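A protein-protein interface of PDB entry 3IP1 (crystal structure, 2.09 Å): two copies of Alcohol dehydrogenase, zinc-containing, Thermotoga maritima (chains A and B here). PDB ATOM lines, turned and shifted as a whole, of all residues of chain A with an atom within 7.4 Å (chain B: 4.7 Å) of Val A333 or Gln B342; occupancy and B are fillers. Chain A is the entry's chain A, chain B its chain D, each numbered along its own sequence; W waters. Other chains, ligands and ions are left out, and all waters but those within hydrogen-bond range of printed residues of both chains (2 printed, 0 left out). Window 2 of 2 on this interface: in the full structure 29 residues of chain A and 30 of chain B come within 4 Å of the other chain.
Of chain B, only His B146 and Gln B342 come within 4 Å of Val A333.
No residue of chain A comes within 4 Å of Gly B343.
Of the printed residues of chain B, Arg A335 touches His B146.
Printed residues of chain B within 4 Å of Ala A336: Gly B340 (3.6 Å).
The nearest residue of chain A that does not touch Gln B342 is Arg A334 (5.8 Å).
A ring nitrogen (ND1) of His B146 is in hydrogen-bond range of the backbone carbonyl oxygen (O) of Val A333 (2.9 Å).
No position is printed for both chains.
Of the 8 pairs that touch across the chains among the printed residues, none has its exchanged pair printed and touching as well.
Water W2 lies within hydrogen-bond range of O of Gln A332, O of Gly B340 and N of Ser B341.
Water W1 lies within hydrogen-bond range of NH1 of Arg A335 and OD1 of Asn B202.
Among the printed residues, merely in contact across the chains: Gln A332 with His B146, Gln A332 with Gly B340, Gln A332 with Ser B341, Gln A332 with Gln B342, Val A333 with Gln B342, Arg A335 with His B146 and Ala A336 with Gly B340.
The backbone carbonyl oxygen (O) of Phe A331 lies within hydrogen-bond range of the backbone NH (N) of Ala A336, at 2.9 Å.
O of Asn B145 is in hydrogen-bond range of NE2 of Gln B342, 2.8 Å away.
The side-chain amide nitrogen of Asn B202 lies within hydrogen-bond range of the side-chain hydroxyl of Ser B341 (3.0 Å).
The side-chain amide nitrogen (ND2) of Asn B202 is in hydrogen-bond range of the backbone carbonyl oxygen (O) of Gln B342 (3.3 Å).
Hydrophobic or aromatic side chains of chain A that line the printed part of chain B: Val A333.
Among the printed residues, no Asp or Glu carboxylate lies within 4 Å of a Lys or Arg side-chain nitrogen of the other chain.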
ATOM      1  N   ILE A 304     -11.078  26.077   2.603  1.00  0.00           N
ATOM      2  CA  ILE A 304     -12.420  25.668   2.983  1.00  0.00           C
ATOM      3  C   ILE A 304     -12.360  25.047   4.384  1.00  0.00           C
ATOM      4  O   ILE A 304     -13.146  25.402   5.262  1.00  0.00           O
ATOM      5  CB  ILE A 304     -13.058  24.693   1.952  1.00  0.00           C
ATOM      6  CG1 ILE A 304     -13.398  25.431   0.637  1.00  0.00           C
ATOM      7  CG2 ILE A 304     -14.319  24.079   2.529  1.00  0.00           C
ATOM      8  CD1 ILE A 304     -13.867  24.483  -0.547  1.00  0.00           C
ATOM      9  N   TRP A 305     -11.394  24.151   4.580  1.00  0.00           N
ATOM     10  CA  TRP A 305     -11.207  23.446   5.839  1.00  0.00           C
ATOM     11  C   TRP A 305     -10.963  24.408   7.000  1.00  0.00           C
ATOM     12  O   TRP A 305     -11.655  24.351   8.003  1.00  0.00           O
ATOM     13  CB  TRP A 305     -10.043  22.463   5.736  1.00  0.00           C
ATOM     14  CG  TRP A 305      -9.861  21.635   6.976  1.00  0.00           C
ATOM     15  CD1 TRP A 305      -8.924  21.816   7.959  1.00  0.00           C
ATOM     16  CD2 TRP A 305     -10.646  20.499   7.371  1.00  0.00           C
ATOM     17  NE1 TRP A 305      -9.071  20.853   8.937  1.00  0.00           N
ATOM     18  CE2 TRP A 305     -10.114  20.030   8.601  1.00  0.00           C
ATOM     19  CE3 TRP A 305     -11.737  19.827   6.801  1.00  0.00           C
ATOM     20  CZ2 TRP A 305     -10.637  18.918   9.270  1.00  0.00           C
ATOM     21  CZ3 TRP A 305     -12.255  18.723   7.459  1.00  0.00           C
ATOM     22  CH2 TRP A 305     -11.709  18.282   8.691  1.00  0.00           C
ATOM     23  N   GLY A 309     -16.367  30.188   7.894  1.00  0.00           N
ATOM     24  CA  GLY A 309     -17.576  30.177   7.061  1.00  0.00           C
ATOM     25  C   GLY A 309     -17.902  28.749   6.653  1.00  0.00           C
ATOM     26  O   GLY A 309     -17.039  27.880   6.640  1.00  0.00           O
ATOM     27  N   ILE A 310     -19.164  28.495   6.355  1.00  0.00           N
ATOM     28  CA  ILE A 310     -19.563  27.188   5.847  1.00  0.00           C
ATOM     29  C   ILE A 310     -20.359  27.419   4.578  1.00  0.00           C
ATOM     30  O   ILE A 310     -20.490  28.561   4.142  1.00  0.00           O
ATOM     31  CB  ILE A 310     -20.377  26.371   6.878  1.00  0.00           C
ATOM     32  CG1 ILE A 310     -21.577  27.174   7.395  1.00  0.00           C
ATOM     33  CG2 ILE A 310     -19.479  25.901   8.020  1.00  0.00           C
ATOM     34  CD1 ILE A 310     -22.592  26.305   8.181  1.00  0.00           C
ATOM     35  N   GLY A 328     -13.239  14.080   0.239  1.00  0.00           N
ATOM     36  CA  GLY A 328     -14.663  14.108   0.597  1.00  0.00           C
ATOM     37  C   GLY A 328     -14.922  14.767   1.943  1.00  0.00           C
ATOM     38  O   GLY A 328     -15.831  15.602   2.077  1.00  0.00           O
ATOM     39  N   GLU A 329     -14.094  14.418   2.925  1.00  0.00           N
ATOM     40  CA  GLU A 329     -14.251  14.882   4.305  1.00  0.00           C
ATOM     41  C   GLU A 329     -14.342  16.392   4.424  1.00  0.00           C
ATOM     42  O   GLU A 329     -15.111  16.914   5.235  1.00  0.00           O
ATOM     43  CB  GLU A 329     -13.086  14.372   5.152  1.00  0.00           C
ATOM     44  CG  GLU A 329     -13.054  14.906   6.584  1.00  0.00           C
ATOM     45  CD  GLU A 329     -12.162  14.084   7.486  1.00  0.00           C
ATOM     46  OE1 GLU A 329     -12.395  12.862   7.568  1.00  0.00           O
ATOM     47  OE2 GLU A 329     -11.237  14.651   8.108  1.00  0.00           O
ATOM     48  N   VAL A 330     -13.530  17.095   3.640  1.00  0.00           N
ATOM     49  CA  VAL A 330     -13.539  18.550   3.660  1.00  0.00           C
ATOM     50  C   VAL A 330     -14.944  19.102   3.374  1.00  0.00           C
ATOM     51  O   VAL A 330     -15.436  19.958   4.121  1.00  0.00           O
ATOM     52  CB  VAL A 330     -12.514  19.120   2.669  1.00  0.00           C
ATOM     53  CG1 VAL A 330     -12.747  20.629   2.451  1.00  0.00           C
ATOM     54  CG2 VAL A 330     -11.047  18.804   3.165  1.00  0.00           C
ATOM     55  N   PHE A 331     -15.567  18.590   2.304  1.00  0.00           N
ATOM     56  CA  PHE A 331     -16.920  18.960   1.889  1.00  0.00           C
ATOM     57  C   PHE A 331     -18.005  18.551   2.876  1.00  0.00           C
ATOM     58  O   PHE A 331     -18.909  19.343   3.128  1.00  0.00           O
ATOM     59  CB  PHE A 331     -17.199  18.559   0.417  1.00  0.00           C
ATOM     60  CG  PHE A 331     -16.326  19.311  -0.531  1.00  0.00           C
ATOM     61  CD1 PHE A 331     -16.786  20.475  -1.144  1.00  0.00           C
ATOM     62  CD2 PHE A 331     -14.983  18.944  -0.700  1.00  0.00           C
ATOM     63  CE1 PHE A 331     -15.934  21.247  -1.954  1.00  0.00           C
ATOM     64  CE2 PHE A 331     -14.133  19.708  -1.503  1.00  0.00           C
ATOM     65  CZ  PHE A 331     -14.608  20.864  -2.128  1.00  0.00           C
ATOM     66  N   GLN A 332     -17.887  17.367   3.476  1.00  0.00           N
ATOM     67  CA  GLN A 332     -18.809  16.958   4.528  1.00  0.00           C
ATOM     68  C   GLN A 332     -18.733  17.860   5.770  1.00  0.00           C
ATOM     69  O   GLN A 332     -19.752  18.368   6.261  1.00  0.00           O
ATOM     70  CB  GLN A 332     -18.549  15.516   4.937  1.00  0.00           C
ATOM     71  CG  GLN A 332     -18.958  14.468   3.899  1.00  0.00           C
ATOM     72  CD  GLN A 332     -18.355  13.092   4.195  1.00  0.00           C
ATOM     73  OE1 GLN A 332     -17.300  12.983   4.831  1.00  0.00           O
ATOM     74  NE2 GLN A 332     -19.013  12.043   3.725  1.00  0.00           N
ATOM     75  N   VAL A 333     -17.517  18.060   6.264  1.00  0.00           N
ATOM     76  CA  VAL A 333     -17.312  18.746   7.522  1.00  0.00           C
ATOM     77  C   VAL A 333     -17.562  20.275   7.439  1.00  0.00           C
ATOM     78  O   VAL A 333     -17.980  20.887   8.422  1.00  0.00           O
ATOM     79  CB  VAL A 333     -15.915  18.398   8.129  1.00  0.00           C
ATOM     80  CG1 VAL A 333     -15.657  19.177   9.422  1.00  0.00           C
ATOM     81  CG2 VAL A 333     -15.804  16.881   8.423  1.00  0.00           C
ATOM     82  N   ARG A 334     -17.310  20.885   6.283  1.00  0.00           N
ATOM     83  CA  ARG A 334     -17.531  22.331   6.142  1.00  0.00           C
ATOM     84  C   ARG A 334     -18.833  22.658   5.408  1.00  0.00           C
ATOM     85  O   ARG A 334     -19.077  23.816   5.041  1.00  0.00           O
ATOM     86  CB  ARG A 334     -16.329  23.012   5.471  1.00  0.00           C
ATOM     87  CG  ARG A 334     -14.963  22.573   6.003  1.00  0.00           C
ATOM     88  CD  ARG A 334     -14.820  22.736   7.532  1.00  0.00           C
ATOM     89  NE  ARG A 334     -14.968  24.131   7.958  1.00  0.00           N
ATOM     90  CZ  ARG A 334     -15.883  24.544   8.830  1.00  0.00           C
ATOM     91  NH1 ARG A 334     -15.954  25.823   9.164  1.00  0.00           N
ATOM     92  NH2 ARG A 334     -16.699  23.666   9.395  1.00  0.00           N
ATOM     93  N   ARG A 335     -19.650  21.633   5.180  1.00  0.00           N
ATOM     94  CA  ARG A 335     -20.950  21.807   4.509  1.00  0.00           C
ATOM     95  C   ARG A 335     -20.786  22.510   3.152  1.00  0.00           C
ATOM     96  O   ARG A 335     -21.512  23.460   2.820  1.00  0.00           O
ATOM     97  CB  ARG A 335     -21.929  22.577   5.427  1.00  0.00           C
ATOM     98  CG  ARG A 335     -23.373  22.170   5.243  1.00  0.00           C
ATOM     99  CD  ARG A 335     -24.310  23.114   6.003  1.00  0.00           C
ATOM    100  NE  ARG A 335     -25.646  22.554   6.076  1.00  0.00           N
ATOM    101  CZ  ARG A 335     -26.620  22.811   5.213  1.00  0.00           C
ATOM    102  NH1 ARG A 335     -27.796  22.222   5.361  1.00  0.00           N
ATOM    103  NH2 ARG A 335     -26.420  23.656   4.215  1.00  0.00           N
ATOM    104  N   ALA A 336     -19.831  22.026   2.372  1.00  0.00           N
ATOM    105  CA  ALA A 336     -19.462  22.673   1.123  1.00  0.00           C
ATOM    106  C   ALA A 336     -19.912  21.830  -0.053  1.00  0.00           C
ATOM    107  O   ALA A 336     -20.306  20.677   0.111  1.00  0.00           O
ATOM    108  CB  ALA A 336     -17.955  22.939   1.080  1.00  0.00           C
ATOM    109  N   ASN B 145     -25.505  21.132  12.449  1.00  0.00           N
ATOM    110  CA  ASN B 145     -24.597  20.008  12.203  1.00  0.00           C
ATOM    111  C   ASN B 145     -23.133  20.467  12.045  1.00  0.00           C
ATOM    112  O   ASN B 145     -22.215  19.649  11.927  1.00  0.00           O
ATOM    113  CB  ASN B 145     -25.045  19.156  11.004  1.00  0.00           C
ATOM    114  CG  ASN B 145     -26.426  18.531  11.200  1.00  0.00           C
ATOM    115  OD1 ASN B 145     -26.632  17.735  12.119  1.00  0.00           O
ATOM    116  ND2 ASN B 145     -27.382  18.885  10.312  1.00  0.00           N
ATOM    117  N   HIS B 146     -22.915  21.778  12.064  1.00  0.00           N
ATOM    118  CA  HIS B 146     -21.574  22.326  11.908  1.00  0.00           C
ATOM    119  C   HIS B 146     -21.226  23.225  13.093  1.00  0.00           C
ATOM    120  O   HIS B 146     -20.374  24.109  13.010  1.00  0.00           O
ATOM    121  CB  HIS B 146     -21.461  22.975  10.520  1.00  0.00           C
ATOM    122  CG  HIS B 146     -21.790  22.005   9.423  1.00  0.00           C
ATOM    123  ND1 HIS B 146     -20.828  21.247   8.785  1.00  0.00           N
ATOM    124  CD2 HIS B 146     -22.987  21.557   8.966  1.00  0.00           C
ATOM    125  CE1 HIS B 146     -21.418  20.430   7.928  1.00  0.00           C
ATOM    126  NE2 HIS B 146     -22.727  20.589   8.029  1.00  0.00           N
ATOM    127  N   ASN B 202     -31.181  13.773   6.171  1.00  0.00           N
ATOM    128  CA  ASN B 202     -30.425  15.001   6.049  1.00  0.00           C
ATOM    129  C   ASN B 202     -29.611  14.947   4.751  1.00  0.00           C
ATOM    130  O   ASN B 202     -29.530  15.927   4.003  1.00  0.00           O
ATOM    131  CB  ASN B 202     -29.525  15.204   7.278  1.00  0.00           C
ATOM    132  CG  ASN B 202     -28.748  16.494   7.217  1.00  0.00           C
ATOM    133  OD1 ASN B 202     -29.314  17.569   7.363  1.00  0.00           O
ATOM    134  ND2 ASN B 202     -27.433  16.399   7.013  1.00  0.00           N
ATOM    135  N   GLY B 340     -21.523  17.305   0.231  1.00  0.00           N
ATOM    136  CA  GLY B 340     -21.202  16.507   1.415  1.00  0.00           C
ATOM    137  C   GLY B 340     -22.388  16.547   2.353  1.00  0.00           C
ATOM    138  O   GLY B 340     -23.230  17.456   2.271  1.00  0.00           O
ATOM    139  N   SER B 341     -22.484  15.566   3.239  1.00  0.00           N
ATOM    140  CA  SER B 341     -23.484  15.621   4.277  1.00  0.00           C
ATOM    141  C   SER B 341     -22.938  15.029   5.570  1.00  0.00           C
ATOM    142  O   SER B 341     -22.152  14.068   5.550  1.00  0.00           O
ATOM    143  CB  SER B 341     -24.771  14.910   3.874  1.00  0.00           C
ATOM    144  OG  SER B 341     -25.752  15.061   4.897  1.00  0.00           O
ATOM    145  N   GLN B 342     -23.377  15.612   6.678  1.00  0.00           N
ATOM    146  CA  GLN B 342     -22.959  15.207   8.009  1.00  0.00           C
ATOM    147  C   GLN B 342     -24.093  15.456   9.006  1.00  0.00           C
ATOM    148  O   GLN B 342     -24.744  16.518   8.971  1.00  0.00           O
ATOM    149  CB  GLN B 342     -21.693  15.994   8.373  1.00  0.00           C
ATOM    150  CG  GLN B 342     -21.576  16.541   9.773  1.00  0.00           C
ATOM    151  CD  GLN B 342     -20.202  17.134   9.998  1.00  0.00           C
ATOM    152  OE1 GLN B 342     -19.209  16.566   9.572  1.00  0.00           O
ATOM    153  NE2 GLN B 342     -20.143  18.282  10.643  1.00  0.00           N
ATOM    154  N   GLY B 343     -24.330  14.471   9.873  1.00  0.00           N
ATOM    155  CA  GLY B 343     -25.216  14.640  11.022  1.00  0.00           C
ATOM    156  C   GLY B 343     -26.688  14.483  10.690  1.00  0.00           C
ATOM    157  O   GLY B 343     -27.044  14.057   9.577  1.00  0.00           O
ATOM    158  N   HIS B 344     -27.543  14.876  11.650  1.00  0.00           N
ATOM    159  CA  HIS B 344     -28.988  14.646  11.579  1.00  0.00           C
ATOM    160  C   HIS B 344     -29.832  15.760  12.251  1.00  0.00           C
ATOM    161  O   HIS B 344     -31.053  15.652  12.347  1.00  0.00           O
ATOM    162  CB  HIS B 344     -29.279  13.313  12.266  1.00  0.00           C
ATOM    163  CG  HIS B 344     -28.715  13.253  13.646  1.00  0.00           C
ATOM    164  ND1 HIS B 344     -27.574  12.543  13.956  1.00  0.00           N
ATOM    165  CD2 HIS B 344     -29.080  13.898  14.781  1.00  0.00           C
ATOM    166  CE1 HIS B 344     -27.289  12.717  15.235  1.00  0.00           C
ATOM    167  NE2 HIS B 344     -28.191  13.528  15.761  1.00  0.00           N
HETATM  168  O   HOH W   1     -27.398  19.692   6.716  1.00  0.00           O
HETATM  169  O   HOH W   2     -22.307  18.505   4.996  1.00  0.00           O
